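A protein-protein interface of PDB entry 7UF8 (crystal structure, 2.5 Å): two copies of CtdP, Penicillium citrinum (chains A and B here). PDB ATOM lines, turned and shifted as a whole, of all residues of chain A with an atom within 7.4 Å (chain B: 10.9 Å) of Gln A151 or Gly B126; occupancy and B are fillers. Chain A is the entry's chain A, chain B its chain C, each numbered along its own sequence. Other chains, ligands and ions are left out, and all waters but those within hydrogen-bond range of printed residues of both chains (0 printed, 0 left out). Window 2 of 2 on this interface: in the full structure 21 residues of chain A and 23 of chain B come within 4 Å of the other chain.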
ATOM      1  N   GLY A 109     -32.048   7.500  -0.024  1.00  0.00           N
ATOM      2  CA  GLY A 109     -31.487   6.164  -0.085  1.00  0.00           C
ATOM      3  C   GLY A 109     -31.661   5.407  -1.393  1.00  0.00           C
ATOM      4  O   GLY A 109     -31.454   4.187  -1.419  1.00  0.00           O
ATOM      5  N   VAL A 110     -32.020   6.080  -2.481  1.00  0.00           N
ATOM      6  CA  VAL A 110     -32.080   5.427  -3.790  1.00  0.00           C
ATOM      7  C   VAL A 110     -30.679   4.899  -4.086  1.00  0.00           C
ATOM      8  O   VAL A 110     -29.714   5.676  -4.058  1.00  0.00           O
ATOM      9  CB  VAL A 110     -32.562   6.393  -4.881  1.00  0.00           C
ATOM     10  CG1 VAL A 110     -32.646   5.672  -6.217  1.00  0.00           C
ATOM     11  CG2 VAL A 110     -33.915   6.984  -4.500  1.00  0.00           C
ATOM     12  N   PRO A 111     -30.507   3.601  -4.365  1.00  0.00           N
ATOM     13  CA  PRO A 111     -29.142   3.063  -4.471  1.00  0.00           C
ATOM     14  C   PRO A 111     -28.509   3.239  -5.845  1.00  0.00           C
ATOM     15  O   PRO A 111     -27.279   3.263  -5.963  1.00  0.00           O
ATOM     16  CB  PRO A 111     -29.328   1.581  -4.121  1.00  0.00           C
ATOM     17  CG  PRO A 111     -30.719   1.266  -4.612  1.00  0.00           C
ATOM     18  CD  PRO A 111     -31.530   2.540  -4.465  1.00  0.00           C
ATOM     19  N   HIS A 112     -29.327   3.353  -6.889  1.00  0.00           N
ATOM     20  CA  HIS A 112     -28.845   3.389  -8.264  1.00  0.00           C
ATOM     21  C   HIS A 112     -29.353   4.647  -8.956  1.00  0.00           C
ATOM     22  O   HIS A 112     -30.559   4.923  -8.957  1.00  0.00           O
ATOM     23  CB  HIS A 112     -29.283   2.136  -9.028  1.00  0.00           C
ATOM     24  CG  HIS A 112     -28.830   0.855  -8.396  1.00  0.00           C
ATOM     25  ND1 HIS A 112     -27.544   0.374  -8.524  1.00  0.00           N
ATOM     26  CD2 HIS A 112     -29.490  -0.040  -7.625  1.00  0.00           C
ATOM     27  CE1 HIS A 112     -27.433  -0.764  -7.862  1.00  0.00           C
ATOM     28  NE2 HIS A 112     -28.601  -1.038  -7.308  1.00  0.00           N
ATOM     29  N   VAL A 113     -28.429   5.413  -9.532  1.00  0.00           N
ATOM     30  CA  VAL A 113     -28.749   6.693 -10.142  1.00  0.00           C
ATOM     31  C   VAL A 113     -28.239   6.706 -11.575  1.00  0.00           C
ATOM     32  O   VAL A 113     -27.107   6.290 -11.850  1.00  0.00           O
ATOM     33  CB  VAL A 113     -28.149   7.869  -9.346  1.00  0.00           C
ATOM     34  CG1 VAL A 113     -28.559   9.195  -9.970  1.00  0.00           C
ATOM     35  CG2 VAL A 113     -28.575   7.799  -7.885  1.00  0.00           C
ATOM     36  N   CYS A 147     -20.605  11.129  -4.163  1.00  0.00           N
ATOM     37  CA  CYS A 147     -21.478  10.753  -3.046  1.00  0.00           C
ATOM     38  C   CYS A 147     -21.196   9.309  -2.645  1.00  0.00           C
ATOM     39  O   CYS A 147     -21.307   8.411  -3.492  1.00  0.00           O
ATOM     40  CB  CYS A 147     -22.944  10.926  -3.428  1.00  0.00           C
ATOM     41  SG  CYS A 147     -24.118  10.456  -2.135  1.00  0.00           S
ATOM     42  N   PRO A 148     -20.833   9.029  -1.388  1.00  0.00           N
ATOM     43  CA  PRO A 148     -20.506   7.646  -1.013  1.00  0.00           C
ATOM     44  C   PRO A 148     -21.717   6.757  -0.782  1.00  0.00           C
ATOM     45  O   PRO A 148     -21.556   5.530  -0.714  1.00  0.00           O
ATOM     46  CB  PRO A 148     -19.701   7.826   0.284  1.00  0.00           C
ATOM     47  CG  PRO A 148     -20.335   9.042   0.927  1.00  0.00           C
ATOM     48  CD  PRO A 148     -20.823   9.932  -0.216  1.00  0.00           C
ATOM     49  N   THR A 149     -22.917   7.326  -0.661  1.00  0.00           N
ATOM     50  CA  THR A 149     -24.092   6.518  -0.347  1.00  0.00           C
ATOM     51  C   THR A 149     -24.561   5.706  -1.550  1.00  0.00           C
ATOM     52  O   THR A 149     -24.980   4.554  -1.397  1.00  0.00           O
ATOM     53  CB  THR A 149     -25.222   7.399   0.190  1.00  0.00           C
ATOM     54  OG1 THR A 149     -25.720   8.252  -0.847  1.00  0.00           O
ATOM     55  CG2 THR A 149     -24.726   8.250   1.347  1.00  0.00           C
ATOM     56  N   PHE A 150     -24.501   6.279  -2.755  1.00  0.00           N
ATOM     57  CA  PHE A 150     -25.036   5.575  -3.918  1.00  0.00           C
ATOM     58  C   PHE A 150     -24.255   4.286  -4.147  1.00  0.00           C
ATOM     59  O   PHE A 150     -23.034   4.243  -3.980  1.00  0.00           O
ATOM     60  CB  PHE A 150     -24.946   6.435  -5.183  1.00  0.00           C
ATOM     61  CG  PHE A 150     -25.818   7.658  -5.172  1.00  0.00           C
ATOM     62  CD1 PHE A 150     -27.059   7.653  -4.557  1.00  0.00           C
ATOM     63  CD2 PHE A 150     -25.400   8.818  -5.807  1.00  0.00           C
ATOM     64  CE1 PHE A 150     -27.855   8.783  -4.564  1.00  0.00           C
ATOM     65  CE2 PHE A 150     -26.191   9.949  -5.817  1.00  0.00           C
ATOM     66  CZ  PHE A 150     -27.420   9.930  -5.198  1.00  0.00           C
ATOM     67  N   GLN A 151     -24.969   3.227  -4.533  1.00  0.00           N
ATOM     68  CA  GLN A 151     -24.293   2.016  -4.986  1.00  0.00           C
ATOM     69  C   GLN A 151     -23.761   2.168  -6.405  1.00  0.00           C
ATOM     70  O   GLN A 151     -22.697   1.632  -6.735  1.00  0.00           O
ATOM     71  CB  GLN A 151     -25.249   0.818  -4.916  1.00  0.00           C
ATOM     72  CG  GLN A 151     -25.230   0.069  -3.591  1.00  0.00           C
ATOM     73  CD  GLN A 151     -24.037  -0.858  -3.462  1.00  0.00           C
ATOM     74  OE1 GLN A 151     -23.363  -0.874  -2.430  1.00  0.00           O
ATOM     75  NE2 GLN A 151     -23.778  -1.645  -4.502  1.00  0.00           N
ATOM     76  N   SER A 152     -24.487   2.893  -7.254  1.00  0.00           N
ATOM     77  CA  SER A 152     -24.037   3.176  -8.605  1.00  0.00           C
ATOM     78  C   SER A 152     -24.537   4.549  -9.020  1.00  0.00           C
ATOM     79  O   SER A 152     -25.679   4.916  -8.730  1.00  0.00           O
ATOM     80  CB  SER A 152     -24.541   2.120  -9.601  1.00  0.00           C
ATOM     81  OG  SER A 152     -25.929   2.266  -9.853  1.00  0.00           O
ATOM     82  N   PHE A 153     -23.681   5.296  -9.712  1.00  0.00           N
ATOM     83  CA  PHE A 153     -24.053   6.583 -10.290  1.00  0.00           C
ATOM     84  C   PHE A 153     -23.471   6.643 -11.692  1.00  0.00           C
ATOM     85  O   PHE A 153     -22.246   6.683 -11.855  1.00  0.00           O
ATOM     86  CB  PHE A 153     -23.556   7.757  -9.452  1.00  0.00           C
ATOM     87  CG  PHE A 153     -23.843   9.093 -10.071  1.00  0.00           C
ATOM     88  CD1 PHE A 153     -25.053   9.726  -9.841  1.00  0.00           C
ATOM     89  CD2 PHE A 153     -22.913   9.711 -10.891  1.00  0.00           C
ATOM     90  CE1 PHE A 153     -25.328  10.951 -10.410  1.00  0.00           C
ATOM     91  CE2 PHE A 153     -23.182  10.937 -11.461  1.00  0.00           C
ATOM     92  CZ  PHE A 153     -24.390  11.560 -11.221  1.00  0.00           C
ATOM     93  N   PRO A 220     -26.248  -1.964 -13.514  1.00  0.00           N
ATOM     94  CA  PRO A 220     -25.727  -0.664 -13.057  1.00  0.00           C
ATOM     95  C   PRO A 220     -24.278  -0.706 -12.594  1.00  0.00           C
ATOM     96  O   PRO A 220     -23.536   0.266 -12.799  1.00  0.00           O
ATOM     97  CB  PRO A 220     -26.688  -0.291 -11.913  1.00  0.00           C
ATOM     98  CG  PRO A 220     -27.286  -1.616 -11.459  1.00  0.00           C
ATOM     99  CD  PRO A 220     -27.412  -2.413 -12.725  1.00  0.00           C
ATOM    100  N   ALA A 221     -23.847  -1.810 -11.977  1.00  0.00           N
ATOM    101  CA  ALA A 221     -22.490  -1.868 -11.442  1.00  0.00           C
ATOM    102  C   ALA A 221     -21.454  -1.759 -12.552  1.00  0.00           C
ATOM    103  O   ALA A 221     -20.416  -1.109 -12.382  1.00  0.00           O
ATOM    104  CB  ALA A 221     -22.297  -3.162 -10.652  1.00  0.00           C
ATOM    105  N   SER A 224     -21.223   1.960 -13.466  1.00  0.00           N
ATOM    106  CA  SER A 224     -21.065   2.971 -12.428  1.00  0.00           C
ATOM    107  C   SER A 224     -19.837   3.825 -12.705  1.00  0.00           C
ATOM    108  O   SER A 224     -18.763   3.306 -13.025  1.00  0.00           O
ATOM    109  CB  SER A 224     -20.951   2.310 -11.055  1.00  0.00           C
ATOM    110  OG  SER A 224     -20.923   3.287 -10.029  1.00  0.00           O
ATOM    111  N   LYS A 225     -20.001   5.141 -12.572  1.00  0.00           N
ATOM    112  CA  LYS A 225     -18.916   6.105 -12.746  1.00  0.00           C
ATOM    113  C   LYS A 225     -18.327   6.072 -14.149  1.00  0.00           C
ATOM    114  O   LYS A 225     -17.201   6.536 -14.364  1.00  0.00           O
ATOM    115  CB  LYS A 225     -17.800   5.877 -11.721  1.00  0.00           C
ATOM    116  CG  LYS A 225     -18.283   5.568 -10.313  1.00  0.00           C
ATOM    117  CD  LYS A 225     -18.901   6.792  -9.659  1.00  0.00           C
ATOM    118  CE  LYS A 225     -19.375   6.488  -8.247  1.00  0.00           C
ATOM    119  NZ  LYS A 225     -18.243   6.276  -7.306  1.00  0.00           N
ATOM    120  N   SER B 120     -10.359   3.679  -9.856  1.00  0.00           N
ATOM    121  CA  SER B 120     -10.586   3.198  -8.498  1.00  0.00           C
ATOM    122  C   SER B 120     -11.613   2.074  -8.557  1.00  0.00           C
ATOM    123  O   SER B 120     -12.785   2.316  -8.865  1.00  0.00           O
ATOM    124  CB  SER B 120     -11.057   4.321  -7.578  1.00  0.00           C
ATOM    125  OG  SER B 120     -11.375   3.805  -6.294  1.00  0.00           O
ATOM    126  N   SER B 121     -11.174   0.850  -8.265  1.00  0.00           N
ATOM    127  CA  SER B 121     -12.119  -0.260  -8.185  1.00  0.00           C
ATOM    128  C   SER B 121     -13.159   0.002  -7.104  1.00  0.00           C
ATOM    129  O   SER B 121     -14.344  -0.301  -7.285  1.00  0.00           O
ATOM    130  CB  SER B 121     -11.377  -1.569  -7.912  1.00  0.00           C
ATOM    131  OG  SER B 121     -10.700  -1.523  -6.668  1.00  0.00           O
ATOM    132  N   HIS B 122     -12.728   0.559  -5.972  1.00  0.00           N
ATOM    133  CA  HIS B 122     -13.658   0.885  -4.896  1.00  0.00           C
ATOM    134  C   HIS B 122     -14.726   1.866  -5.365  1.00  0.00           C
ATOM    135  O   HIS B 122     -15.922   1.666  -5.121  1.00  0.00           O
ATOM    136  CB  HIS B 122     -12.890   1.463  -3.707  1.00  0.00           C
ATOM    137  CG  HIS B 122     -13.768   1.901  -2.573  1.00  0.00           C
ATOM    138  ND1 HIS B 122     -13.897   1.176  -1.409  1.00  0.00           N
ATOM    139  CD2 HIS B 122     -14.556   2.992  -2.425  1.00  0.00           C
ATOM    140  CE1 HIS B 122     -14.728   1.801  -0.592  1.00  0.00           C
ATOM    141  NE2 HIS B 122     -15.143   2.905  -1.188  1.00  0.00           N
ATOM    142  N   ALA B 123     -14.310   2.940  -6.039  1.00  0.00           N
ATOM    143  CA  ALA B 123     -15.264   3.970  -6.437  1.00  0.00           C
ATOM    144  C   ALA B 123     -16.257   3.449  -7.468  1.00  0.00           C
ATOM    145  O   ALA B 123     -17.430   3.838  -7.461  1.00  0.00           O
ATOM    146  CB  ALA B 123     -14.520   5.191  -6.976  1.00  0.00           C
ATOM    147  N   LEU B 124     -15.808   2.576  -8.369  1.00  0.00           N
ATOM    148  CA  LEU B 124     -16.671   2.106  -9.443  1.00  0.00           C
ATOM    149  C   LEU B 124     -17.557   0.935  -9.038  1.00  0.00           C
ATOM    150  O   LEU B 124     -18.607   0.734  -9.655  1.00  0.00           O
ATOM    151  CB  LEU B 124     -15.825   1.713 -10.656  1.00  0.00           C
ATOM    152  CG  LEU B 124     -15.459   2.842 -11.623  1.00  0.00           C
ATOM    153  CD1 LEU B 124     -14.970   4.063 -10.853  1.00  0.00           C
ATOM    154  CD2 LEU B 124     -14.417   2.371 -12.626  1.00  0.00           C
ATOM    155  N   SER B 125     -17.165   0.159  -8.030  1.00  0.00           N
ATOM    156  CA  SER B 125     -17.880  -1.051  -7.650  1.00  0.00           C
ATOM    157  C   SER B 125     -18.757  -0.855  -6.419  1.00  0.00           C
ATOM    158  O   SER B 125     -19.282  -1.833  -5.880  1.00  0.00           O
ATOM    159  CB  SER B 125     -16.886  -2.191  -7.408  1.00  0.00           C
ATOM    160  OG  SER B 125     -16.115  -1.961  -6.241  1.00  0.00           O
ATOM    161  N   GLY B 126     -18.931   0.384  -5.971  1.00  0.00           N
ATOM    162  CA  GLY B 126     -19.719   0.645  -4.779  1.00  0.00           C
ATOM    163  C   GLY B 126     -19.147   0.073  -3.499  1.00  0.00           C
ATOM    164  O   GLY B 126     -19.913  -0.259  -2.586  1.00  0.00           O
ATOM    165  N   GLY B 127     -17.809  -0.061  -3.410  1.00  0.00           N
ATOM    166  CA  GLY B 127     -17.122  -0.481  -2.160  1.00  0.00           C
ATOM    167  C   GLY B 127     -16.912  -1.988  -2.026  1.00  0.00           C
ATOM    168  O   GLY B 127     -16.198  -2.391  -1.067  1.00  0.00           O
ATOM    169  N   LYS B 128     -17.462  -2.825  -2.928  1.00  0.00           N
ATOM    170  CA  LYS B 128     -17.367  -4.319  -2.804  1.00  0.00           C
ATOM    171  C   LYS B 128     -15.981  -4.771  -3.298  1.00  0.00           C
ATOM    172  O   LYS B 128     -15.690  -5.981  -3.121  1.00  0.00           O
ATOM    173  CB  LYS B 128     -18.508  -5.064  -3.537  1.00  0.00           C
ATOM    174  CG  LYS B 128     -18.434  -5.131  -5.074  1.00  0.00           C
ATOM    175  CD  LYS B 128     -19.649  -5.910  -5.689  1.00  0.00           C
ATOM    176  CE  LYS B 128     -19.895  -5.622  -7.177  1.00  0.00           C
ATOM    177  NZ  LYS B 128     -20.454  -4.233  -7.401  1.00  0.00           N
ATOM    178  N   PHE B 129     -15.167  -3.895  -3.919  1.00  0.00           N
ATOM    179  CA  PHE B 129     -13.756  -4.196  -4.319  1.00  0.00           C
ATOM    180  C   PHE B 129     -12.814  -3.128  -3.737  1.00  0.00           C
ATOM    181  O   PHE B 129     -13.294  -2.032  -3.399  1.00  0.00           O
ATOM    182  CB  PHE B 129     -13.481  -4.299  -5.839  1.00  0.00           C
ATOM    183  CG  PHE B 129     -14.192  -5.404  -6.596  1.00  0.00           C
ATOM    184  CD1 PHE B 129     -14.231  -6.701  -6.097  1.00  0.00           C
ATOM    185  CD2 PHE B 129     -14.752  -5.170  -7.849  1.00  0.00           C
ATOM    186  CE1 PHE B 129     -14.853  -7.725  -6.803  1.00  0.00           C
ATOM    187  CE2 PHE B 129     -15.373  -6.194  -8.556  1.00  0.00           C
ATOM    188  CZ  PHE B 129     -15.424  -7.472  -8.035  1.00  0.00           C
ATOM    189  N   ASN B 130     -11.538  -3.462  -3.570  1.00  0.00           N
ATOM    190  CA  ASN B 130     -10.474  -2.589  -3.049  1.00  0.00           C
ATOM    191  C   ASN B 130      -9.135  -3.070  -3.603  1.00  0.00           C
ATOM    192  O   ASN B 130      -8.627  -4.122  -3.194  1.00  0.00           O
ATOM    193  CB  ASN B 130     -10.428  -2.551  -1.510  1.00  0.00           C
ATOM    194  CG  ASN B 130     -10.168  -1.136  -0.960  1.00  0.00           C
ATOM    195  OD1 ASN B 130     -10.856  -0.184  -1.330  1.00  0.00           O
ATOM    196  ND2 ASN B 130      -9.171  -1.000  -0.085  1.00  0.00           N
ATOM    197  N   THR B 131      -8.557  -2.284  -4.513  1.00  0.00           N
ATOM    198  CA  THR B 131      -7.312  -2.615  -5.210  1.00  0.00           C
ATOM    199  C   THR B 131      -6.408  -1.401  -5.037  1.00  0.00           C
ATOM    200  O   THR B 131      -6.356  -0.519  -5.904  1.00  0.00           O
ATOM    201  CB  THR B 131      -7.563  -2.931  -6.685  1.00  0.00           C
ATOM    202  OG1 THR B 131      -8.344  -1.887  -7.286  1.00  0.00           O
ATOM    203  CG2 THR B 131      -8.310  -4.253  -6.829  1.00  0.00           C
ATOM    204  N   ASP B 135      -6.180   2.184  -6.841  1.00  0.00           N
ATOM    205  CA  ASP B 135      -7.031   3.177  -6.195  1.00  0.00           C
ATOM    206  C   ASP B 135      -6.231   4.359  -5.655  1.00  0.00           C
ATOM    207  O   ASP B 135      -6.764   5.468  -5.570  1.00  0.00           O
ATOM    208  CB  ASP B 135      -7.835   2.519  -5.070  1.00  0.00           C
ATOM    209  CG  ASP B 135      -8.794   1.446  -5.575  1.00  0.00           C
ATOM    210  OD1 ASP B 135      -8.802   1.173  -6.793  1.00  0.00           O
ATOM    211  OD2 ASP B 135      -9.539   0.874  -4.749  1.00  0.00           O
ATOM    212  N   GLN B 275      -8.361  -9.371  -7.143  1.00  0.00           N
ATOM    213  CA  GLN B 275      -9.373  -8.292  -7.116  1.00  0.00           C
ATOM    214  C   GLN B 275      -9.294  -7.399  -8.358  1.00  0.00           C
ATOM    215  O   GLN B 275     -10.329  -6.963  -8.883  1.00  0.00           O
ATOM    216  CB  GLN B 275      -9.260  -7.437  -5.843  1.00  0.00           C
ATOM    217  CG  GLN B 275      -9.552  -8.279  -4.606  1.00  0.00           C
ATOM    218  CD  GLN B 275     -10.334  -7.554  -3.519  1.00  0.00           C
ATOM    219  OE1 GLN B 275     -11.317  -6.862  -3.790  1.00  0.00           O
ATOM    220  NE2 GLN B 275      -9.921  -7.753  -2.274  1.00  0.00           N
ATOM    221  N   PHE B 279     -12.403  -7.114 -10.903  1.00  0.00           N
ATOM    222  CA  PHE B 279     -12.935  -5.806 -11.263  1.00  0.00           C
ATOM    223  C   PHE B 279     -12.926  -5.614 -12.774  1.00  0.00           C
ATOM    224  O   PHE B 279     -13.899  -5.115 -13.352  1.00  0.00           O
ATOM    225  CB  PHE B 279     -12.119  -4.715 -10.571  1.00  0.00           C
ATOM    226  CG  PHE B 279     -12.346  -3.342 -11.125  1.00  0.00           C
ATOM    227  CD1 PHE B 279     -13.596  -2.751 -11.053  1.00  0.00           C
ATOM    228  CD2 PHE B 279     -11.307  -2.637 -11.713  1.00  0.00           C
ATOM    229  CE1 PHE B 279     -13.808  -1.486 -11.560  1.00  0.00           C
ATOM    230  CE2 PHE B 279     -11.514  -1.373 -12.224  1.00  0.00           C
ATOM    231  CZ  PHE B 279     -12.766  -0.796 -12.147  1.00  0.00           C
ATOM    232  N   MET B 282     -15.694  -7.781 -14.231  1.00  0.00           N
ATOM    233  CA  MET B 282     -16.975  -7.166 -13.914  1.00  0.00           C
ATOM    234  C   MET B 282     -17.259  -5.998 -14.848  1.00  0.00           C
ATOM    235  O   MET B 282     -18.410  -5.701 -15.154  1.00  0.00           O
ATOM    236  CB  MET B 282     -16.993  -6.685 -12.463  1.00  0.00           C
ATOM    237  CG  MET B 282     -18.350  -6.197 -11.987  1.00  0.00           C
ATOM    238  SD  MET B 282     -18.471  -4.251 -11.897  1.00  0.00           S
ATOM    239  CE  MET B 282     -18.113  -4.016  -9.988  1.00  0.00           C
ATOM    240  N   ARG B 283     -16.196  -5.333 -15.293  1.00  0.00           N
ATOM    241  CA  ARG B 283     -16.306  -4.205 -16.203  1.00  0.00           C
ATOM    242  C   ARG B 283     -16.293  -4.631 -17.663  1.00  0.00           C
ATOM    243  O   ARG B 283     -16.106  -3.784 -18.542  1.00  0.00           O
ATOM    244  CB  ARG B 283     -15.171  -3.211 -15.943  1.00  0.00           C
ATOM    245  CG  ARG B 283     -15.239  -2.524 -14.587  1.00  0.00           C
ATOM    246  CD  ARG B 283     -16.526  -1.729 -14.413  1.00  0.00           C
ATOM    247  NE  ARG B 283     -16.393  -0.367 -14.917  1.00  0.00           N
ATOM    248  CZ  ARG B 283     -17.058   0.676 -14.440  1.00  0.00           C
ATOM    249  NH1 ARG B 283     -17.918   0.552 -13.443  1.00  0.00           N
ATOM    250  NH2 ARG B 283     -16.849   1.878 -14.972  1.00  0.00           N
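The backbone carbonyl oxygen (O) of Ala A221 is in hydrogen-bond range of the guanidinium group (NH1) of Arg B283 (3.2 Å).
The backbone carbonyl oxygen of Leu B124 sits close to the side-chain hydroxyl of Ser A224 (3.5 Å).
O of Ser A224 lies within hydrogen-bond range of NH1 of Arg B283, 2.9 Å away.
NZ of Lys A225 is in hydrogen-bond range of O of Ala B123.
O of Ala A221 sits close to SD of Met B282 (3.7 Å).
No residue of chain B comes within 4 Å of Pro A111.
Of chain B, only Gly B126 (3.5 Å) comes within 4 Å of Gln A151.
No residue of chain B comes within 4 Å of Ser A152.
Printed residues of chain B within 4 Å of Ala A221: Leu B124, Lys B128, Met B282 and Arg B283.
Of the printed residues of chain A, Leu B124 touches Ala A221 (3.8 Å), Ser A224 (3.2 Å) and Lys A225 (3.5 Å).
Ser B125 touches none of the printed residues of chain A.
Printed residues of chain A within 4 Å of Lys B128: Ala A221.
The nearest residue of chain B that does not touch Gln A151 is Ser B125 (4.7 Å).
Among the printed residues, 9 pairs touch across the chains.
Gln A151 touches Gly B126.
O of Ala A221 touches O of Leu B124, at 3.8 Å.
CB of Ala A221 touches NZ of Lys B128, 3.9 Å away.
Lys A225 touches Leu B124 (CB to CD1, 3.5 Å).
The backbone NH (N) of Gln A151 lies within hydrogen-bond range of the backbone carbonyl oxygen (O) of Pro A111, at 2.7 Å.
The side-chain hydroxyl of Ser A224 lies within hydrogen-bond range of the backbone NH of Phe A153 (3.4 Å).
O of Phe A153 lies within hydrogen-bond range of N of Lys A225 (2.8 Å).
The side-chain hydroxyl (OG) of Ser B120 sits at hydrogen-bond distance from the backbone NH (N) of Ala B123 (3.1 Å).
O of Ser B125 is in hydrogen-bond range of NZ of Lys B128, at 3.1 Å.
No position is printed for both chains.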
